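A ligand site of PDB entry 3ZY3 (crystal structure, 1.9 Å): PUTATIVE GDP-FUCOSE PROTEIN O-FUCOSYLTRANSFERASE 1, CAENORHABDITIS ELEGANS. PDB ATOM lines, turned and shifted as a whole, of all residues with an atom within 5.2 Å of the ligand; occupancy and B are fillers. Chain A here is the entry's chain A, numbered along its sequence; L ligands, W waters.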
ATOM      1  N   GLY A  18      -5.576  12.315 -19.275  1.00  0.00           N
ATOM      2  CA  GLY A  18      -5.967  13.685 -19.600  1.00  0.00           C
ATOM      3  C   GLY A  18      -4.814  14.653 -19.625  1.00  0.00           C
ATOM      4  O   GLY A  18      -3.636  14.277 -19.492  1.00  0.00           O
ATOM      5  N   ARG A  19      -5.153  15.934 -19.772  1.00  0.00           N
ATOM      6  CA  ARG A  19      -4.151  16.979 -19.853  1.00  0.00           C
ATOM      7  C   ARG A  19      -3.949  17.683 -18.511  1.00  0.00           C
ATOM      8  O   ARG A  19      -4.287  17.081 -17.472  1.00  0.00           O
ATOM      9  CB  ARG A  19      -4.495  17.893 -21.015  1.00  0.00           C
ATOM     10  CG  ARG A  19      -4.133  17.163 -22.324  1.00  0.00           C
ATOM     11  CD  ARG A  19      -4.485  17.971 -23.544  1.00  0.00           C
ATOM     12  NE  ARG A  19      -5.922  18.141 -23.663  1.00  0.00           N
ATOM     13  CZ  ARG A  19      -6.496  18.894 -24.596  1.00  0.00           C
ATOM     14  NH1 ARG A  19      -5.747  19.530 -25.492  1.00  0.00           N
ATOM     15  NH2 ARG A  19      -7.819  18.998 -24.632  1.00  0.00           N
ATOM     16  N   PHE A  20      -3.396  18.906 -18.475  1.00  0.00           N
ATOM     17  CA  PHE A  20      -2.854  19.469 -17.225  1.00  0.00           C
ATOM     18  C   PHE A  20      -3.873  19.599 -16.083  1.00  0.00           C
ATOM     19  O   PHE A  20      -3.579  19.226 -14.918  1.00  0.00           O
ATOM     20  CB  PHE A  20      -2.137  20.813 -17.486  1.00  0.00           C
ATOM     21  CG  PHE A  20      -1.336  21.311 -16.317  1.00  0.00           C
ATOM     22  CD1 PHE A  20      -0.254  20.595 -15.822  1.00  0.00           C
ATOM     23  CD2 PHE A  20      -1.661  22.529 -15.722  1.00  0.00           C
ATOM     24  CE1 PHE A  20       0.490  21.088 -14.747  1.00  0.00           C
ATOM     25  CE2 PHE A  20      -0.942  23.027 -14.648  1.00  0.00           C
ATOM     26  CZ  PHE A  20       0.140  22.311 -14.153  1.00  0.00           C
ATOM     27  N   GLY A  21      -5.067  20.110 -16.410  1.00  0.00           N
ATOM     28  CA  GLY A  21      -6.198  20.159 -15.467  1.00  0.00           C
ATOM     29  C   GLY A  21      -6.510  18.811 -14.862  1.00  0.00           C
ATOM     30  O   GLY A  21      -6.628  18.700 -13.632  1.00  0.00           O
ATOM     31  N   ASN A  22      -6.680  17.807 -15.725  1.00  0.00           N
ATOM     32  CA  ASN A  22      -6.844  16.392 -15.326  1.00  0.00           C
ATOM     33  C   ASN A  22      -5.712  15.946 -14.380  1.00  0.00           C
ATOM     34  O   ASN A  22      -5.971  15.325 -13.343  1.00  0.00           O
ATOM     35  CB  ASN A  22      -6.773  15.531 -16.587  1.00  0.00           C
ATOM     36  CG  ASN A  22      -8.076  14.815 -16.953  1.00  0.00           C
ATOM     37  OD1 ASN A  22      -8.889  15.335 -17.726  1.00  0.00           O
ATOM     38  ND2 ASN A  22      -8.206  13.559 -16.509  1.00  0.00           N
ATOM     39  N   HIS A 217     -11.577  32.591 -18.773  1.00  0.00           N
ATOM     40  CA  HIS A 217     -11.074  31.385 -19.404  1.00  0.00           C
ATOM     41  C   HIS A 217     -12.078  30.985 -20.497  1.00  0.00           C
ATOM     42  O   HIS A 217     -13.216  30.727 -20.197  1.00  0.00           O
ATOM     43  CB  HIS A 217     -10.889  30.256 -18.405  1.00  0.00           C
ATOM     44  CG  HIS A 217     -10.425  28.975 -19.037  1.00  0.00           C
ATOM     45  ND1 HIS A 217     -10.851  27.731 -18.625  1.00  0.00           N
ATOM     46  CD2 HIS A 217      -9.624  28.757 -20.112  1.00  0.00           C
ATOM     47  CE1 HIS A 217     -10.294  26.802 -19.378  1.00  0.00           C
ATOM     48  NE2 HIS A 217      -9.543  27.403 -20.296  1.00  0.00           N
ATOM     49  N   LEU A 218     -11.653  31.000 -21.762  1.00  0.00           N
ATOM     50  CA  LEU A 218     -12.522  30.565 -22.859  1.00  0.00           C
ATOM     51  C   LEU A 218     -12.052  29.219 -23.371  1.00  0.00           C
ATOM     52  O   LEU A 218     -11.078  29.130 -24.101  1.00  0.00           O
ATOM     53  CB  LEU A 218     -12.575  31.596 -24.002  1.00  0.00           C
ATOM     54  CG  LEU A 218     -12.931  33.048 -23.643  1.00  0.00           C
ATOM     55  CD1 LEU A 218     -13.001  33.914 -24.916  1.00  0.00           C
ATOM     56  CD2 LEU A 218     -14.280  33.048 -22.952  1.00  0.00           C
ATOM     57  N   ARG A 219     -12.804  28.183 -22.975  1.00  0.00           N
ATOM     58  CA  ARG A 219     -12.542  26.807 -23.316  1.00  0.00           C
ATOM     59  C   ARG A 219     -13.351  26.500 -24.576  1.00  0.00           C
ATOM     60  O   ARG A 219     -14.595  26.476 -24.522  1.00  0.00           O
ATOM     61  CB  ARG A 219     -12.986  25.923 -22.131  1.00  0.00           C
ATOM     62  CG  ARG A 219     -12.665  24.436 -22.265  1.00  0.00           C
ATOM     63  CD  ARG A 219     -11.131  24.122 -22.381  1.00  0.00           C
ATOM     64  NE  ARG A 219     -10.863  22.684 -22.208  1.00  0.00           N
ATOM     65  CZ  ARG A 219     -10.894  21.773 -23.169  1.00  0.00           C
ATOM     66  NH1 ARG A 219     -11.166  22.121 -24.430  1.00  0.00           N
ATOM     67  NH2 ARG A 219     -10.687  20.484 -22.886  1.00  0.00           N
ATOM     68  N   ASP A 223     -12.557  19.562 -28.889  1.00  0.00           N
ATOM     69  CA  ASP A 223     -12.906  18.478 -27.991  1.00  0.00           C
ATOM     70  C   ASP A 223     -14.056  18.859 -27.062  1.00  0.00           C
ATOM     71  O   ASP A 223     -14.704  17.988 -26.499  1.00  0.00           O
ATOM     72  CB  ASP A 223     -11.683  18.021 -27.174  1.00  0.00           C
ATOM     73  CG  ASP A 223     -11.174  19.088 -26.202  1.00  0.00           C
ATOM     74  OD1 ASP A 223     -10.826  20.203 -26.629  1.00  0.00           O
ATOM     75  OD2 ASP A 223     -11.104  18.806 -24.995  1.00  0.00           O
ATOM     76  N   TRP A 224     -14.308  20.168 -26.921  1.00  0.00           N
ATOM     77  CA  TRP A 224     -15.306  20.650 -25.976  1.00  0.00           C
ATOM     78  C   TRP A 224     -16.770  20.336 -26.306  1.00  0.00           C
ATOM     79  O   TRP A 224     -17.567  20.129 -25.394  1.00  0.00           O
ATOM     80  CB  TRP A 224     -15.159  22.156 -25.768  1.00  0.00           C
ATOM     81  CG  TRP A 224     -15.686  22.635 -24.453  1.00  0.00           C
ATOM     82  CD1 TRP A 224     -16.680  23.538 -24.260  1.00  0.00           C
ATOM     83  CD2 TRP A 224     -15.257  22.218 -23.139  1.00  0.00           C
ATOM     84  NE1 TRP A 224     -16.882  23.737 -22.916  1.00  0.00           N
ATOM     85  CE2 TRP A 224     -16.020  22.953 -22.199  1.00  0.00           C
ATOM     86  CE3 TRP A 224     -14.286  21.327 -22.675  1.00  0.00           C
ATOM     87  CZ2 TRP A 224     -15.873  22.783 -20.811  1.00  0.00           C
ATOM     88  CZ3 TRP A 224     -14.111  21.174 -21.290  1.00  0.00           C
ATOM     89  CH2 TRP A 224     -14.904  21.906 -20.380  1.00  0.00           C
ATOM     90  N   ALA A 286      -7.552  34.030 -21.440  1.00  0.00           N
ATOM     91  CA  ALA A 286      -6.821  32.787 -21.678  1.00  0.00           C
ATOM     92  C   ALA A 286      -7.728  31.890 -22.489  1.00  0.00           C
ATOM     93  O   ALA A 286      -8.928  31.746 -22.177  1.00  0.00           O
ATOM     94  CB  ALA A 286      -6.489  32.125 -20.345  1.00  0.00           C
ATOM     95  N   SER A 287      -7.208  31.287 -23.555  1.00  0.00           N
ATOM     96  CA  SER A 287      -8.013  30.358 -24.356  1.00  0.00           C
ATOM     97  C   SER A 287      -7.163  29.259 -24.949  1.00  0.00           C
ATOM     98  O   SER A 287      -5.970  29.479 -25.173  1.00  0.00           O
ATOM     99  CB  SER A 287      -8.735  31.062 -25.505  1.00  0.00           C
ATOM    100  OG  SER A 287      -9.581  30.106 -26.144  1.00  0.00           O
ATOM    101  N   ASP A 288      -7.777  28.109 -25.191  1.00  0.00           N
ATOM    102  CA  ASP A 288      -7.127  26.998 -25.902  1.00  0.00           C
ATOM    103  C   ASP A 288      -7.223  27.160 -27.422  1.00  0.00           C
ATOM    104  O   ASP A 288      -6.500  26.491 -28.193  1.00  0.00           O
ATOM    105  CB  ASP A 288      -7.667  25.614 -25.467  1.00  0.00           C
ATOM    106  CG  ASP A 288      -9.212  25.509 -25.528  1.00  0.00           C
ATOM    107  OD1 ASP A 288      -9.907  26.512 -25.736  1.00  0.00           O
ATOM    108  OD2 ASP A 288      -9.717  24.374 -25.403  1.00  0.00           O
ATOM    109  N   ASP A 313      -0.111  31.912 -26.285  1.00  0.00           N
ATOM    110  CA  ASP A 313      -0.787  31.650 -25.030  1.00  0.00           C
ATOM    111  C   ASP A 313      -0.134  30.418 -24.368  1.00  0.00           C
ATOM    112  O   ASP A 313      -0.351  29.248 -24.787  1.00  0.00           O
ATOM    113  CB  ASP A 313      -2.304  31.480 -25.288  1.00  0.00           C
ATOM    114  CG  ASP A 313      -3.127  31.337 -24.004  1.00  0.00           C
ATOM    115  OD1 ASP A 313      -2.766  30.526 -23.127  1.00  0.00           O
ATOM    116  OD2 ASP A 313      -4.163  32.016 -23.904  1.00  0.00           O
ATOM    117  N   ASP A 314       0.707  30.695 -23.373  1.00  0.00           N
ATOM    118  CA  ASP A 314       1.367  29.661 -22.579  1.00  0.00           C
ATOM    119  C   ASP A 314       0.417  29.300 -21.471  1.00  0.00           C
ATOM    120  O   ASP A 314       0.032  30.197 -20.674  1.00  0.00           O
ATOM    121  CB  ASP A 314       2.659  30.209 -21.950  1.00  0.00           C
ATOM    122  CG  ASP A 314       3.360  29.179 -21.097  1.00  0.00           C
ATOM    123  OD1 ASP A 314       4.123  28.383 -21.673  1.00  0.00           O
ATOM    124  OD2 ASP A 314       3.115  29.119 -19.877  1.00  0.00           O
ATOM    125  N   MET A 315       0.024  28.028 -21.391  1.00  0.00           N
ATOM    126  CA  MET A 315      -1.032  27.580 -20.453  1.00  0.00           C
ATOM    127  C   MET A 315      -0.707  27.805 -18.973  1.00  0.00           C
ATOM    128  O   MET A 315      -1.605  28.086 -18.164  1.00  0.00           O
ATOM    129  CB  MET A 315      -1.427  26.098 -20.704  1.00  0.00           C
ATOM    130  CG  MET A 315      -0.564  25.057 -19.979  1.00  0.00           C
ATOM    131  SD  MET A 315      -1.054  23.331 -20.310  1.00  0.00           S
ATOM    132  CE  MET A 315      -0.100  23.120 -21.804  1.00  0.00           C
ATOM    133  N   SER A 318      -0.741  31.519 -18.249  1.00  0.00           N
ATOM    134  CA  SER A 318      -2.159  31.883 -18.296  1.00  0.00           C
ATOM    135  C   SER A 318      -2.890  31.572 -17.003  1.00  0.00           C
ATOM    136  O   SER A 318      -3.647  32.412 -16.541  1.00  0.00           O
ATOM    137  CB  SER A 318      -2.877  31.251 -19.486  1.00  0.00           C
ATOM    138  OG  SER A 318      -2.617  32.023 -20.639  1.00  0.00           O
ATOM    139  N   MET A 322      -4.546  34.379 -14.445  1.00  0.00           N
ATOM    140  CA  MET A 322      -5.932  34.271 -13.985  1.00  0.00           C
ATOM    141  C   MET A 322      -5.993  34.177 -12.452  1.00  0.00           C
ATOM    142  O   MET A 322      -6.893  34.737 -11.839  1.00  0.00           O
ATOM    143  CB  MET A 322      -6.668  33.105 -14.654  1.00  0.00           C
ATOM    144  CG  MET A 322      -6.807  33.263 -16.165  1.00  0.00           C
ATOM    145  SD  MET A 322      -7.842  32.004 -16.917  1.00  0.00           S
ATOM    146  CE  MET A 322      -6.716  30.580 -16.996  1.00  0.00           C
ATOM    147  N   VAL A 333     -17.172  23.611 -15.907  1.00  0.00           N
ATOM    148  CA  VAL A 333     -16.938  22.196 -16.235  1.00  0.00           C
ATOM    149  C   VAL A 333     -15.423  21.894 -16.354  1.00  0.00           C
ATOM    150  O   VAL A 333     -14.971  20.772 -16.077  1.00  0.00           O
ATOM    151  CB  VAL A 333     -17.745  21.833 -17.504  1.00  0.00           C
ATOM    152  CG1 VAL A 333     -17.426  20.435 -18.002  1.00  0.00           C
ATOM    153  CG2 VAL A 333     -19.268  21.997 -17.212  1.00  0.00           C
ATOM    154  N   SER A 334     -14.639  22.904 -16.687  1.00  0.00           N
ATOM    155  CA  SER A 334     -13.228  22.764 -16.963  1.00  0.00           C
ATOM    156  C   SER A 334     -12.376  22.556 -15.715  1.00  0.00           C
ATOM    157  O   SER A 334     -12.402  23.403 -14.791  1.00  0.00           O
ATOM    158  CB  SER A 334     -12.693  23.987 -17.708  1.00  0.00           C
ATOM    159  OG  SER A 334     -11.296  23.844 -17.879  1.00  0.00           O
ATOM    160  N   THR A 335     -11.586  21.465 -15.700  1.00  0.00           N
ATOM    161  CA  THR A 335     -10.617  21.228 -14.613  1.00  0.00           C
ATOM    162  C   THR A 335      -9.451  22.212 -14.710  1.00  0.00           C
ATOM    163  O   THR A 335      -8.766  22.459 -13.721  1.00  0.00           O
ATOM    164  CB  THR A 335     -10.075  19.778 -14.594  1.00  0.00           C
ATOM    165  OG1 THR A 335      -9.372  19.509 -15.831  1.00  0.00           O
ATOM    166  CG2 THR A 335     -11.229  18.794 -14.436  1.00  0.00           C
ATOM    167  N   PHE A 336      -9.196  22.735 -15.918  1.00  0.00           N
ATOM    168  CA  PHE A 336      -8.200  23.823 -16.107  1.00  0.00           C
ATOM    169  C   PHE A 336      -8.666  25.081 -15.331  1.00  0.00           C
ATOM    170  O   PHE A 336      -7.945  25.611 -14.522  1.00  0.00           O
ATOM    171  CB  PHE A 336      -8.048  24.090 -17.621  1.00  0.00           C
ATOM    172  CG  PHE A 336      -6.879  24.984 -17.991  1.00  0.00           C
ATOM    173  CD1 PHE A 336      -5.610  24.451 -18.178  1.00  0.00           C
ATOM    174  CD2 PHE A 336      -7.079  26.338 -18.225  1.00  0.00           C
ATOM    175  CE1 PHE A 336      -4.508  25.275 -18.559  1.00  0.00           C
ATOM    176  CE2 PHE A 336      -5.993  27.182 -18.622  1.00  0.00           C
ATOM    177  CZ  PHE A 336      -4.732  26.655 -18.806  1.00  0.00           C
HETATM  178  P1  LIG L   1     -10.369  20.499 -19.126  1.00  0.00           P
HETATM  179  O1  LIG L   1     -10.359  19.588 -20.325  1.00  0.00           O
HETATM  180  O2  LIG L   1     -10.881  21.857 -19.549  1.00  0.00           O
HETATM  181  O3  LIG L   1     -11.027  19.912 -17.911  1.00  0.00           O
HETATM  182  O4  LIG L   1      -8.854  20.803 -18.719  1.00  0.00           O
HETATM  183  P2  LIG L   1      -7.477  20.020 -19.055  1.00  0.00           P
HETATM  184  O5  LIG L   1      -7.462  18.691 -18.378  1.00  0.00           O
HETATM  185  O6  LIG L   1      -6.358  20.914 -18.537  1.00  0.00           O
HETATM  186  O7  LIG L   1      -7.373  19.855 -20.642  1.00  0.00           O
HETATM  187  C1  LIG L   1      -7.476  21.019 -21.450  1.00  0.00           C
HETATM  188  C2  LIG L   1      -6.116  21.325 -22.059  1.00  0.00           C
HETATM  189  O8  LIG L   1      -6.336  22.223 -23.122  1.00  0.00           O
HETATM  190  C3  LIG L   1      -5.173  22.111 -21.161  1.00  0.00           C
HETATM  191  O9  LIG L   1      -4.440  21.318 -20.233  1.00  0.00           O
HETATM  192  C4  LIG L   1      -4.294  22.826 -22.184  1.00  0.00           C
HETATM  193  O10 LIG L   1      -3.375  21.927 -22.837  1.00  0.00           O
HETATM  194  C5  LIG L   1      -5.351  23.266 -23.174  1.00  0.00           C
HETATM  195  N1  LIG L   1      -5.963  24.540 -22.683  1.00  0.00           N
HETATM  196  C6  LIG L   1      -7.204  24.681 -22.132  1.00  0.00           C
HETATM  197  N2  LIG L   1      -7.445  25.968 -21.819  1.00  0.00           N
HETATM  198  C7  LIG L   1      -6.332  26.679 -22.168  1.00  0.00           C
HETATM  199  C8  LIG L   1      -5.874  28.084 -22.107  1.00  0.00           C
HETATM  200  O11 LIG L   1      -6.644  28.944 -21.618  1.00  0.00           O
HETATM  201  N3  LIG L   1      -4.641  28.390 -22.582  1.00  0.00           N
HETATM  202  C9  LIG L   1      -3.811  27.444 -23.117  1.00  0.00           C
HETATM  203  N4  LIG L   1      -2.567  27.765 -23.598  1.00  0.00           N
HETATM  204  N5  LIG L   1      -4.166  26.142 -23.217  1.00  0.00           N
HETATM  205  C10 LIG L   1      -5.376  25.719 -22.737  1.00  0.00           C
HETATM  206  O   HOH W   1      -7.891  16.617 -20.073  1.00  0.00           O
HETATM  207  O   HOH W   2     -13.313  19.243 -18.387  1.00  0.00           O
HETATM  208  O   HOH W   3      -9.244  17.932 -22.091  1.00  0.00           O
HETATM  209  O   HOH W   4      -1.801  19.876 -21.077  1.00  0.00           O
HETATM  210  O   HOH W   5      -1.777  23.039 -24.690  1.00  0.00           O
HETATM  211  O   HOH W   6      -8.012  22.159 -25.603  1.00  0.00           O
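Water W2 bridges O3 of the ligand (2.4 Å) and O of Val 333 (3.2 Å).
Water W3 lies within hydrogen-bond range of an oxygen (O1) of the ligand (2.7 Å), the guanidinium group of Arg 219 (3.0 Å) and the guanidinium group of Arg 19 (3.1 Å).
Water W1 lies within hydrogen-bond range of an oxygen (O5) of the ligand, the backbone NH (N) of Arg 19 and the side-chain amide oxygen (OD1) of Asn 22.
Water W6 lies within hydrogen-bond range of OD2 of Asp 288 (2.8 Å), O8 of the ligand (3.0 Å), NH2 of Arg 19 (3.3 Å) and NH1 of Arg 219 (3.4 Å).
Water W4 lies within hydrogen-bond range of O9 of the ligand (3.1 Å), N of Phe 20 (3.2 Å) and SD of Met 315 (3.6 Å).
Arg 19 touches the ligand.
Trp 224 touches the ligand (CZ3 to O2, 3.7 Å).
C of Ala 286 touches O11 of the ligand, 3.3 Å away.
Asp 288 touches the ligand (CB to N1, 3.4 Å).
C of Asp 314 touches N4 of the ligand, 3.97 Å away.
Hydrophobic or aromatic side chains that line the ligand: Phe 20, His 217, Trp 224, Ala 286, Met 315 and Phe 336.
Of the 22 residues printed, 16 come within 4 Å of the ligand.
The nearest printed residue that does not touch the ligand is Val 333 (4.4 Å).
The side-chain hydroxyl (OG1) of Thr 335 is in hydrogen-bond range of the backbone NH (N) of Asn 22 (3.2 Å).
N of Ser 287 sits at hydrogen-bond distance from OD2 of Asp 313, 3.2 Å away.
OD2 of Asp 288 lies within salt-bridge range of NH1 of Arg 219 (2.8 Å).
OD2 of Asp 223 lies within salt-bridge range of NH2 of Arg 19, at 3.3 Å.
NH2 of Arg 219 lies within salt-bridge range of OD2 of Asp 223.
The backbone carbonyl oxygen of Asp 314 sits at hydrogen-bond distance from the side-chain hydroxyl of Ser 318 (3.2 Å).
N of Phe 336 lies within hydrogen-bond range of OG of Ser 334, 3.1 Å away.
OG of Ser 287 sits at hydrogen-bond distance from O of Leu 218, at 2.7 Å.
A nitrogen (N4) of the ligand is in hydrogen-bond range of the side-chain carboxylate (OD1) of Asp 313, at 2.8 Å.
N of Ser 287 is in hydrogen-bond range of O11 of the ligand, 3.1 Å away.
The backbone NH (N) of Gly 21 lies within hydrogen-bond range of an oxygen (O6) of the ligand, at 2.6 Å.
The side-chain hydroxyl of Thr 335 sits at hydrogen-bond distance from an oxygen (O3) of the ligand (2.7 Å).
A nitrogen (N4) of the ligand lies within hydrogen-bond range of the backbone carbonyl oxygen (O) of Asp 313 (2.9 Å).
N of Phe 20 is in hydrogen-bond range of O9 of the ligand.
N of Thr 335 lies within hydrogen-bond range of O3 of the ligand, at 2.8 Å.
The backbone carbonyl oxygen of Ser 287 lies within hydrogen-bond range of a nitrogen (N3) of the ligand (3.1 Å).
NH2 of Arg 219 is in salt-bridge range of O1 of the ligand.
The backbone NH (N) of Asn 22 is in hydrogen-bond range of an oxygen (O5) of the ligand, at 2.9 Å.
N of Phe 336 is in hydrogen-bond range of O4 of the ligand, 3.4 Å away.
A ring nitrogen (NE2) of His 217 is in hydrogen-bond range of a nitrogen (N2) of the ligand, 3.0 Å away.
An oxygen (O10) of the ligand sits close to the side-chain sulfur (SD) of Met 315, at 3.7 Å.
OG of Ser 334 lies within hydrogen-bond range of O2 of the ligand (2.6 Å).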
